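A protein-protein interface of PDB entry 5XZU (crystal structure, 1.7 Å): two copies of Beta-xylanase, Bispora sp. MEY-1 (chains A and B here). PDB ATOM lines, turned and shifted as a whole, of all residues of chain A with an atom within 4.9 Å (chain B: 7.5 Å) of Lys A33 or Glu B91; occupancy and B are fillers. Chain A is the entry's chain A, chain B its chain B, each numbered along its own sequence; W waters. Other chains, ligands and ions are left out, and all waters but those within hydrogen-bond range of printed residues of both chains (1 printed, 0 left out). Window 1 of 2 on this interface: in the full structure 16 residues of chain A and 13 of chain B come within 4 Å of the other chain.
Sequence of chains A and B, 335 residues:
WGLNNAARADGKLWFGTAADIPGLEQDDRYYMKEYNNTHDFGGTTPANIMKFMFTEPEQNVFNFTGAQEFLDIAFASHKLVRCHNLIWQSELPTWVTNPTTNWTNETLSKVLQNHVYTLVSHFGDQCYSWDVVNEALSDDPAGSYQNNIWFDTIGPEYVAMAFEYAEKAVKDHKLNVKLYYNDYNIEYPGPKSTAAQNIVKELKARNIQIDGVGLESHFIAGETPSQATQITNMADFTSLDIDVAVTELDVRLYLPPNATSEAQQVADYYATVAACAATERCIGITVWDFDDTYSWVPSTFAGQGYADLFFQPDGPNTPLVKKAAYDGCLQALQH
The side-chain carboxylate of Glu B91 is in salt-bridge range of the side-chain amino group of Lys A33, 3.8 Å away.
The side-chain carboxylate (OD2) of Asp B20 is in salt-bridge range of the guanidinium group (NH1) of Arg A29 (2.9 Å).
The side-chain amino group (NZ) of Lys B51 lies within hydrogen-bond range of the side-chain amide oxygen (OD1) of Asn B48 (3.3 Å).
NZ of Lys B51 is in salt-bridge range of OE2 of Glu B91 (3.1 Å).
O of Glu B91 sits close to N of Met B53 (3.4 Å).
OD1 of Asn B48 lies close to OE2 of Glu B91 (3.5 Å).
The side-chain amide nitrogen (ND2) of Asn B48 sits at hydrogen-bond distance from the side-chain carboxylate (OD1) of Asp B20 (2.9 Å).
Lys A33 touches Asn B48.
Of chain B, only Asn B48 (3.6 Å) and Glu B91 (3.3 Å) come within 4 Å of Lys A33.
Printed residues of chain A within 4 Å of Asp B20: Arg A29 (2.9 Å).
Of the printed residues of chain A, Asn B48 touches Lys A33 (3.6 Å).
Glu B91 touches just one residue of chain A: Lys A33 (3.3 Å).
The nearest printed residue of chain A that does not touch Glu B91 is Asn A37 (7.9 Å).
Of the 9 printed residues of chain A, 2 touch a printed residue of chain B.
Of the 16 printed residues of chain B, 3 touch a printed residue of chain A.
Among the printed residues, Asp or Glu carboxylates within 4 Å of a Lys or Arg side-chain nitrogen of the other chain: Arg A29 with Asp B20 (2.9 Å) and Lys A33 with Glu B91 (3.8 Å).
No position is printed for both chains.
Water W1 bridges the side-chain carboxylate of Asp B20 (2.5 Å) and the side-chain hydroxyl of Tyr A30 (2.6 Å).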
ATOM      1  N   ARG A  29       3.407 -11.250  31.195  1.00  0.00           N
ATOM      2  CA  ARG A  29       4.610 -10.970  30.447  1.00  0.00           C
ATOM      3  C   ARG A  29       5.763 -11.910  30.886  1.00  0.00           C
ATOM      4  O   ARG A  29       6.643 -12.227  30.076  1.00  0.00           O
ATOM      5  CB  ARG A  29       5.003  -9.464  30.542  1.00  0.00           C
ATOM      6  CG  ARG A  29       5.599  -8.989  31.866  1.00  0.00           C
ATOM      7  CD  ARG A  29       6.240  -7.584  31.772  1.00  0.00           C
ATOM      8  NE  ARG A  29       7.714  -7.666  31.797  1.00  0.00           N
ATOM      9  CZ  ARG A  29       8.527  -7.001  32.634  1.00  0.00           C
ATOM     10  NH1 ARG A  29       9.848  -7.215  32.587  1.00  0.00           N
ATOM     11  NH2 ARG A  29       8.050  -6.098  33.498  1.00  0.00           N
ATOM     12  N   TYR A  30       5.734 -12.393  32.127  1.00  0.00           N
ATOM     13  CA  TYR A  30       6.799 -13.268  32.609  1.00  0.00           C
ATOM     14  C   TYR A  30       6.609 -14.689  32.057  1.00  0.00           C
ATOM     15  O   TYR A  30       7.553 -15.332  31.634  1.00  0.00           O
ATOM     16  CB  TYR A  30       6.790 -13.309  34.124  1.00  0.00           C
ATOM     17  CG  TYR A  30       7.168 -11.991  34.768  1.00  0.00           C
ATOM     18  CD1 TYR A  30       8.479 -11.595  34.831  1.00  0.00           C
ATOM     19  CD2 TYR A  30       6.195 -11.138  35.260  1.00  0.00           C
ATOM     20  CE1 TYR A  30       8.817 -10.324  35.254  1.00  0.00           C
ATOM     21  CE2 TYR A  30       6.532  -9.898  35.796  1.00  0.00           C
ATOM     22  CZ  TYR A  30       7.841  -9.495  35.779  1.00  0.00           C
ATOM     23  OH  TYR A  30       8.197  -8.271  36.290  1.00  0.00           O
ATOM     24  N   TYR A  31       5.362 -15.117  31.979  1.00  0.00           N
ATOM     25  CA  TYR A  31       5.018 -16.350  31.266  1.00  0.00           C
ATOM     26  C   TYR A  31       5.384 -16.279  29.801  1.00  0.00           C
ATOM     27  O   TYR A  31       6.098 -17.148  29.323  1.00  0.00           O
ATOM     28  CB  TYR A  31       3.530 -16.679  31.431  1.00  0.00           C
ATOM     29  CG  TYR A  31       3.094 -17.948  30.715  1.00  0.00           C
ATOM     30  CD1 TYR A  31       2.783 -17.924  29.375  1.00  0.00           C
ATOM     31  CD2 TYR A  31       3.078 -19.179  31.374  1.00  0.00           C
ATOM     32  CE1 TYR A  31       2.477 -19.102  28.692  1.00  0.00           C
ATOM     33  CE2 TYR A  31       2.792 -20.366  30.694  1.00  0.00           C
ATOM     34  CZ  TYR A  31       2.474 -20.309  29.351  1.00  0.00           C
ATOM     35  OH  TYR A  31       2.170 -21.461  28.642  1.00  0.00           O
ATOM     36  N   MET A  32       4.969 -15.218  29.106  1.00  0.00           N
ATOM     37  CA  MET A  32       5.180 -15.128  27.681  1.00  0.00           C
ATOM     38  C   MET A  32       6.655 -15.018  27.320  1.00  0.00           C
ATOM     39  O   MET A  32       7.031 -15.505  26.282  1.00  0.00           O
ATOM     40  CB  MET A  32       4.358 -14.013  27.011  1.00  0.00           C
ATOM     41  CG  MET A  32       2.857 -14.220  27.024  1.00  0.00           C
ATOM     42  SD  MET A  32       2.289 -15.772  26.267  1.00  0.00           S
ATOM     43  CE  MET A  32       2.781 -15.549  24.571  1.00  0.00           C
ATOM     44  N   LYS A  33       7.473 -14.327  28.130  1.00  0.00           N
ATOM     45  CA  LYS A  33       8.898 -14.216  27.840  1.00  0.00           C
ATOM     46  C   LYS A  33       9.519 -15.627  27.767  1.00  0.00           C
ATOM     47  O   LYS A  33      10.276 -15.944  26.857  1.00  0.00           O
ATOM     48  CB  LYS A  33       9.570 -13.408  28.934  1.00  0.00           C
ATOM     49  CG  LYS A  33      11.057 -13.228  28.723  1.00  0.00           C
ATOM     50  CD  LYS A  33      11.559 -12.033  29.523  1.00  0.00           C
ATOM     51  CE  LYS A  33      13.005 -11.711  29.192  1.00  0.00           C
ATOM     52  NZ  LYS A  33      13.482 -10.569  30.022  1.00  0.00           N
ATOM     53  N   GLU A  34       9.111 -16.497  28.678  1.00  0.00           N
ATOM     54  CA  GLU A  34       9.632 -17.866  28.703  1.00  0.00           C
ATOM     55  C   GLU A  34       9.003 -18.764  27.635  1.00  0.00           C
ATOM     56  O   GLU A  34       9.711 -19.573  27.021  1.00  0.00           O
ATOM     57  CB  GLU A  34       9.446 -18.481  30.090  1.00  0.00           C
ATOM     58  CG  GLU A  34       9.857 -19.946  30.265  1.00  0.00           C
ATOM     59  CD  GLU A  34      11.234 -20.344  29.741  1.00  0.00           C
ATOM     60  OE1 GLU A  34      12.123 -19.488  29.555  1.00  0.00           O
ATOM     61  OE2 GLU A  34      11.462 -21.580  29.632  1.00  0.00           O
ATOM     62  N   TYR A  35       7.707 -18.590  27.365  1.00  0.00           N
ATOM     63  CA  TYR A  35       7.073 -19.288  26.223  1.00  0.00           C
ATOM     64  C   TYR A  35       7.800 -18.976  24.923  1.00  0.00           C
ATOM     65  O   TYR A  35       8.038 -19.851  24.085  1.00  0.00           O
ATOM     66  CB  TYR A  35       5.585 -18.915  26.110  1.00  0.00           C
ATOM     67  CG  TYR A  35       4.855 -19.640  25.014  1.00  0.00           C
ATOM     68  CD1 TYR A  35       4.590 -20.997  25.122  1.00  0.00           C
ATOM     69  CD2 TYR A  35       4.529 -18.996  23.832  1.00  0.00           C
ATOM     70  CE1 TYR A  35       3.913 -21.661  24.129  1.00  0.00           C
ATOM     71  CE2 TYR A  35       3.881 -19.667  22.793  1.00  0.00           C
ATOM     72  CZ  TYR A  35       3.594 -21.002  22.936  1.00  0.00           C
ATOM     73  OH  TYR A  35       2.965 -21.682  21.905  1.00  0.00           O
ATOM     74  N   ASN A  36       8.194 -17.716  24.774  1.00  0.00           N
ATOM     75  CA  ASN A  36       8.764 -17.257  23.526  1.00  0.00           C
ATOM     76  C   ASN A  36      10.256 -17.641  23.462  1.00  0.00           C
ATOM     77  O   ASN A  36      10.929 -17.395  22.471  1.00  0.00           O
ATOM     78  CB  ASN A  36       8.599 -15.734  23.409  1.00  0.00           C
ATOM     79  CG  ASN A  36       7.158 -15.294  23.062  1.00  0.00           C
ATOM     80  OD1 ASN A  36       6.267 -16.090  22.757  1.00  0.00           O
ATOM     81  ND2 ASN A  36       6.940 -14.001  23.118  1.00  0.00           N
ATOM     82  N   ASN A  37      10.785 -18.213  24.531  1.00  0.00           N
ATOM     83  CA  ASN A  37      12.215 -18.505  24.605  1.00  0.00           C
ATOM     84  C   ASN A  37      12.551 -19.786  23.819  1.00  0.00           C
ATOM     85  O   ASN A  37      12.360 -20.882  24.331  1.00  0.00           O
ATOM     86  CB  ASN A  37      12.615 -18.634  26.068  1.00  0.00           C
ATOM     87  CG  ASN A  37      14.054 -19.074  26.267  1.00  0.00           C
ATOM     88  OD1 ASN A  37      14.877 -18.990  25.374  1.00  0.00           O
ATOM     89  ND2 ASN A  37      14.338 -19.591  27.442  1.00  0.00           N
ATOM     90  N   ASP B  20      14.406  -3.058  36.478  1.00  0.00           N
ATOM     91  CA  ASP B  20      13.527  -3.496  35.395  1.00  0.00           C
ATOM     92  C   ASP B  20      12.319  -2.571  35.314  1.00  0.00           C
ATOM     93  O   ASP B  20      11.209  -2.920  35.749  1.00  0.00           O
ATOM     94  CB  ASP B  20      13.087  -4.927  35.678  1.00  0.00           C
ATOM     95  CG  ASP B  20      12.349  -5.551  34.519  1.00  0.00           C
ATOM     96  OD1 ASP B  20      12.549  -5.120  33.369  1.00  0.00           O
ATOM     97  OD2 ASP B  20      11.647  -6.554  34.762  1.00  0.00           O
ATOM     98  N   ALA B  47      17.175  -2.526  32.784  1.00  0.00           N
ATOM     99  CA  ALA B  47      17.363  -3.987  32.617  1.00  0.00           C
ATOM    100  C   ALA B  47      16.881  -4.496  31.262  1.00  0.00           C
ATOM    101  O   ALA B  47      17.428  -5.473  30.742  1.00  0.00           O
ATOM    102  CB  ALA B  47      16.688  -4.759  33.750  1.00  0.00           C
ATOM    103  N   ASN B  48      15.853  -3.860  30.696  1.00  0.00           N
ATOM    104  CA  ASN B  48      15.218  -4.369  29.462  1.00  0.00           C
ATOM    105  C   ASN B  48      14.753  -3.319  28.436  1.00  0.00           C
ATOM    106  O   ASN B  48      14.849  -3.546  27.222  1.00  0.00           O
ATOM    107  CB  ASN B  48      14.025  -5.250  29.818  1.00  0.00           C
ATOM    108  CG  ASN B  48      14.431  -6.588  30.350  1.00  0.00           C
ATOM    109  OD1 ASN B  48      15.068  -7.369  29.660  1.00  0.00           O
ATOM    110  ND2 ASN B  48      14.135  -6.827  31.613  1.00  0.00           N
ATOM    111  N   LYS B  51      16.553  -2.275  25.038  1.00  0.00           N
ATOM    112  CA  LYS B  51      17.003  -3.289  24.109  1.00  0.00           C
ATOM    113  C   LYS B  51      16.289  -3.196  22.759  1.00  0.00           C
ATOM    114  O   LYS B  51      15.318  -2.446  22.592  1.00  0.00           O
ATOM    115  CB  LYS B  51      16.819  -4.654  24.749  1.00  0.00           C
ATOM    116  CG  LYS B  51      17.821  -4.903  25.865  1.00  0.00           C
ATOM    117  CD  LYS B  51      17.493  -6.144  26.677  1.00  0.00           C
ATOM    118  CE  LYS B  51      18.628  -6.429  27.655  1.00  0.00           C
ATOM    119  NZ  LYS B  51      18.218  -7.470  28.618  1.00  0.00           N
ATOM    120  N   PHE B  52      16.831  -3.925  21.784  1.00  0.00           N
ATOM    121  CA  PHE B  52      16.411  -3.843  20.375  1.00  0.00           C
ATOM    122  C   PHE B  52      14.907  -4.103  20.193  1.00  0.00           C
ATOM    123  O   PHE B  52      14.227  -3.342  19.506  1.00  0.00           O
ATOM    124  CB  PHE B  52      17.256  -4.825  19.544  1.00  0.00           C
ATOM    125  CG  PHE B  52      17.355  -4.494  18.074  1.00  0.00           C
ATOM    126  CD1 PHE B  52      16.250  -4.646  17.238  1.00  0.00           C
ATOM    127  CD2 PHE B  52      18.577  -4.170  17.506  1.00  0.00           C
ATOM    128  CE1 PHE B  52      16.356  -4.415  15.880  1.00  0.00           C
ATOM    129  CE2 PHE B  52      18.692  -3.962  16.137  1.00  0.00           C
ATOM    130  CZ  PHE B  52      17.578  -4.075  15.335  1.00  0.00           C
ATOM    131  N   MET B  53      14.365  -5.142  20.831  1.00  0.00           N
ATOM    132  CA  MET B  53      12.980  -5.520  20.566  1.00  0.00           C
ATOM    133  C   MET B  53      12.016  -4.427  21.019  1.00  0.00           C
ATOM    134  O   MET B  53      10.928  -4.265  20.439  1.00  0.00           O
ATOM    135  CB  MET B  53      12.615  -6.862  21.200  1.00  0.00           C
ATOM    136  CG  MET B  53      12.626  -6.903  22.714  1.00  0.00           C
ATOM    137  SD  MET B  53      12.163  -8.533  23.337  1.00  0.00           S
ATOM    138  CE  MET B  53      10.453  -8.223  23.802  1.00  0.00           C
ATOM    139  N   PHE B  54      12.439  -3.650  22.014  1.00  0.00           N
ATOM    140  CA  PHE B  54      11.591  -2.608  22.574  1.00  0.00           C
ATOM    141  C   PHE B  54      11.734  -1.274  21.831  1.00  0.00           C
ATOM    142  O   PHE B  54      10.750  -0.551  21.653  1.00  0.00           O
ATOM    143  CB  PHE B  54      11.889  -2.416  24.047  1.00  0.00           C
ATOM    144  CG  PHE B  54      11.546  -3.606  24.889  1.00  0.00           C
ATOM    145  CD1 PHE B  54      10.229  -3.857  25.247  1.00  0.00           C
ATOM    146  CD2 PHE B  54      12.543  -4.469  25.341  1.00  0.00           C
ATOM    147  CE1 PHE B  54       9.910  -4.940  26.059  1.00  0.00           C
ATOM    148  CE2 PHE B  54      12.221  -5.587  26.100  1.00  0.00           C
ATOM    149  CZ  PHE B  54      10.910  -5.800  26.493  1.00  0.00           C
ATOM    150  N   ASN B  85      21.047  -2.014  25.690  1.00  0.00           N
ATOM    151  CA  ASN B  85      22.262  -1.992  24.898  1.00  0.00           C
ATOM    152  C   ASN B  85      21.798  -1.914  23.440  1.00  0.00           C
ATOM    153  O   ASN B  85      20.624  -2.148  23.168  1.00  0.00           O
ATOM    154  CB  ASN B  85      23.062  -3.288  25.111  1.00  0.00           C
ATOM    155  CG  ASN B  85      22.308  -4.520  24.656  1.00  0.00           C
ATOM    156  OD1 ASN B  85      21.869  -4.604  23.499  1.00  0.00           O
ATOM    157  ND2 ASN B  85      22.098  -5.459  25.570  1.00  0.00           N
ATOM    158  N   TRP B  88      23.127  -6.942  20.392  1.00  0.00           N
ATOM    159  CA  TRP B  88      23.196  -8.115  21.278  1.00  0.00           C
ATOM    160  C   TRP B  88      22.505  -9.268  20.543  1.00  0.00           C
ATOM    161  O   TRP B  88      21.531  -9.046  19.819  1.00  0.00           O
ATOM    162  CB  TRP B  88      22.415  -7.833  22.564  1.00  0.00           C
ATOM    163  CG  TRP B  88      22.477  -8.905  23.627  1.00  0.00           C
ATOM    164  CD1 TRP B  88      23.577  -9.627  23.994  1.00  0.00           C
ATOM    165  CD2 TRP B  88      21.469  -9.205  24.594  1.00  0.00           C
ATOM    166  NE1 TRP B  88      23.312 -10.371  25.114  1.00  0.00           N
ATOM    167  CE2 TRP B  88      22.025 -10.131  25.502  1.00  0.00           C
ATOM    168  CE3 TRP B  88      20.154  -8.776  24.791  1.00  0.00           C
ATOM    169  CZ2 TRP B  88      21.294 -10.678  26.539  1.00  0.00           C
ATOM    170  CZ3 TRP B  88      19.442  -9.296  25.841  1.00  0.00           C
ATOM    171  CH2 TRP B  88      19.998 -10.274  26.675  1.00  0.00           C
ATOM    172  N   GLN B  89      22.944 -10.497  20.791  1.00  0.00           N
ATOM    173  CA  GLN B  89      22.343 -11.650  20.119  1.00  0.00           C
ATOM    174  C   GLN B  89      20.898 -11.936  20.485  1.00  0.00           C
ATOM    175  O   GLN B  89      20.187 -12.537  19.692  1.00  0.00           O
ATOM    176  CB  GLN B  89      23.168 -12.897  20.377  1.00  0.00           C
ATOM    177  CG  GLN B  89      23.138 -13.377  21.813  1.00  0.00           C
ATOM    178  CD  GLN B  89      23.262 -14.881  21.892  1.00  0.00           C
ATOM    179  OE1 GLN B  89      24.314 -15.404  22.227  1.00  0.00           O
ATOM    180  NE2 GLN B  89      22.199 -15.582  21.519  1.00  0.00           N
ATOM    181  N   SER B  90      20.475 -11.584  21.700  1.00  0.00           N
ATOM    182  CA  SER B  90      19.205 -12.067  22.257  1.00  0.00           C
ATOM    183  C   SER B  90      18.148 -10.972  22.225  1.00  0.00           C
ATOM    184  O   SER B  90      18.450  -9.806  21.951  1.00  0.00           O
ATOM    185  CB  SER B  90      19.383 -12.519  23.716  1.00  0.00           C
ATOM    186  OG  SER B  90      20.451 -13.429  23.841  1.00  0.00           O
ATOM    187  N   GLU B  91      16.928 -11.320  22.619  1.00  0.00           N
ATOM    188  CA  GLU B  91      15.903 -10.301  22.827  1.00  0.00           C
ATOM    189  C   GLU B  91      15.761  -9.458  21.545  1.00  0.00           C
ATOM    190  O   GLU B  91      15.739  -8.213  21.579  1.00  0.00           O
ATOM    191  CB  GLU B  91      16.272  -9.417  24.028  1.00  0.00           C
ATOM    192  CG  GLU B  91      15.175  -9.274  25.072  1.00  0.00           C
ATOM    193  CD  GLU B  91      15.521  -9.971  26.368  1.00  0.00           C
ATOM    194  OE1 GLU B  91      15.000 -11.079  26.601  1.00  0.00           O
ATOM    195  OE2 GLU B  91      16.339  -9.425  27.138  1.00  0.00           O
ATOM    196  N   LEU B  92      15.736 -10.154  20.409  1.00  0.00           N
ATOM    197  CA  LEU B  92      15.543  -9.510  19.117  1.00  0.00           C
ATOM    198  C   LEU B  92      14.123  -9.752  18.623  1.00  0.00           C
ATOM    199  O   LEU B  92      13.543 -10.823  18.849  1.00  0.00           O
ATOM    200  CB  LEU B  92      16.562  -9.997  18.081  1.00  0.00           C
ATOM    201  CG  LEU B  92      18.040  -9.711  18.361  1.00  0.00           C
ATOM    202  CD1 LEU B  92      18.961 -10.222  17.267  1.00  0.00           C
ATOM    203  CD2 LEU B  92      18.254  -8.217  18.540  1.00  0.00           C
ATOM    204  N   PRO B  93      13.544  -8.735  17.973  1.00  0.00           N
ATOM    205  CA  PRO B  93      12.163  -8.804  17.506  1.00  0.00           C
ATOM    206  C   PRO B  93      11.986  -9.780  16.329  1.00  0.00           C
ATOM    207  O   PRO B  93      12.954 -10.089  15.606  1.00  0.00           O
ATOM    208  CB  PRO B  93      11.888  -7.367  17.080  1.00  0.00           C
ATOM    209  CG  PRO B  93      13.222  -6.862  16.609  1.00  0.00           C
ATOM    210  CD  PRO B  93      14.240  -7.525  17.488  1.00  0.00           C
ATOM    211  N   THR B  94      10.771 -10.306  16.157  1.00  0.00           N
ATOM    212  CA  THR B  94      10.581 -11.387  15.183  1.00  0.00           C
ATOM    213  C   THR B  94      10.735 -10.880  13.748  1.00  0.00           C
ATOM    214  O   THR B  94      11.137 -11.639  12.876  1.00  0.00           O
ATOM    215  CB  THR B  94       9.270 -12.184  15.394  1.00  0.00           C
ATOM    216  OG1 THR B  94       8.143 -11.308  15.360  1.00  0.00           O
ATOM    217  CG2 THR B  94       9.291 -12.907  16.743  1.00  0.00           C
ATOM    218  N   THR B  97      14.564 -11.954  13.638  1.00  0.00           N
ATOM    219  CA  THR B  97      14.831 -13.396  13.847  1.00  0.00           C
ATOM    220  C   THR B  97      14.034 -14.245  12.856  1.00  0.00           C
ATOM    221  O   THR B  97      14.501 -15.283  12.391  1.00  0.00           O
ATOM    222  CB  THR B  97      14.439 -13.879  15.269  1.00  0.00           C
ATOM    223  OG1 THR B  97      13.029 -13.699  15.481  1.00  0.00           O
ATOM    224  CG2 THR B  97      15.222 -13.148  16.346  1.00  0.00           C
HETATM  225  O   HOH W   1      10.628  -7.459  36.841  1.00  0.00           O
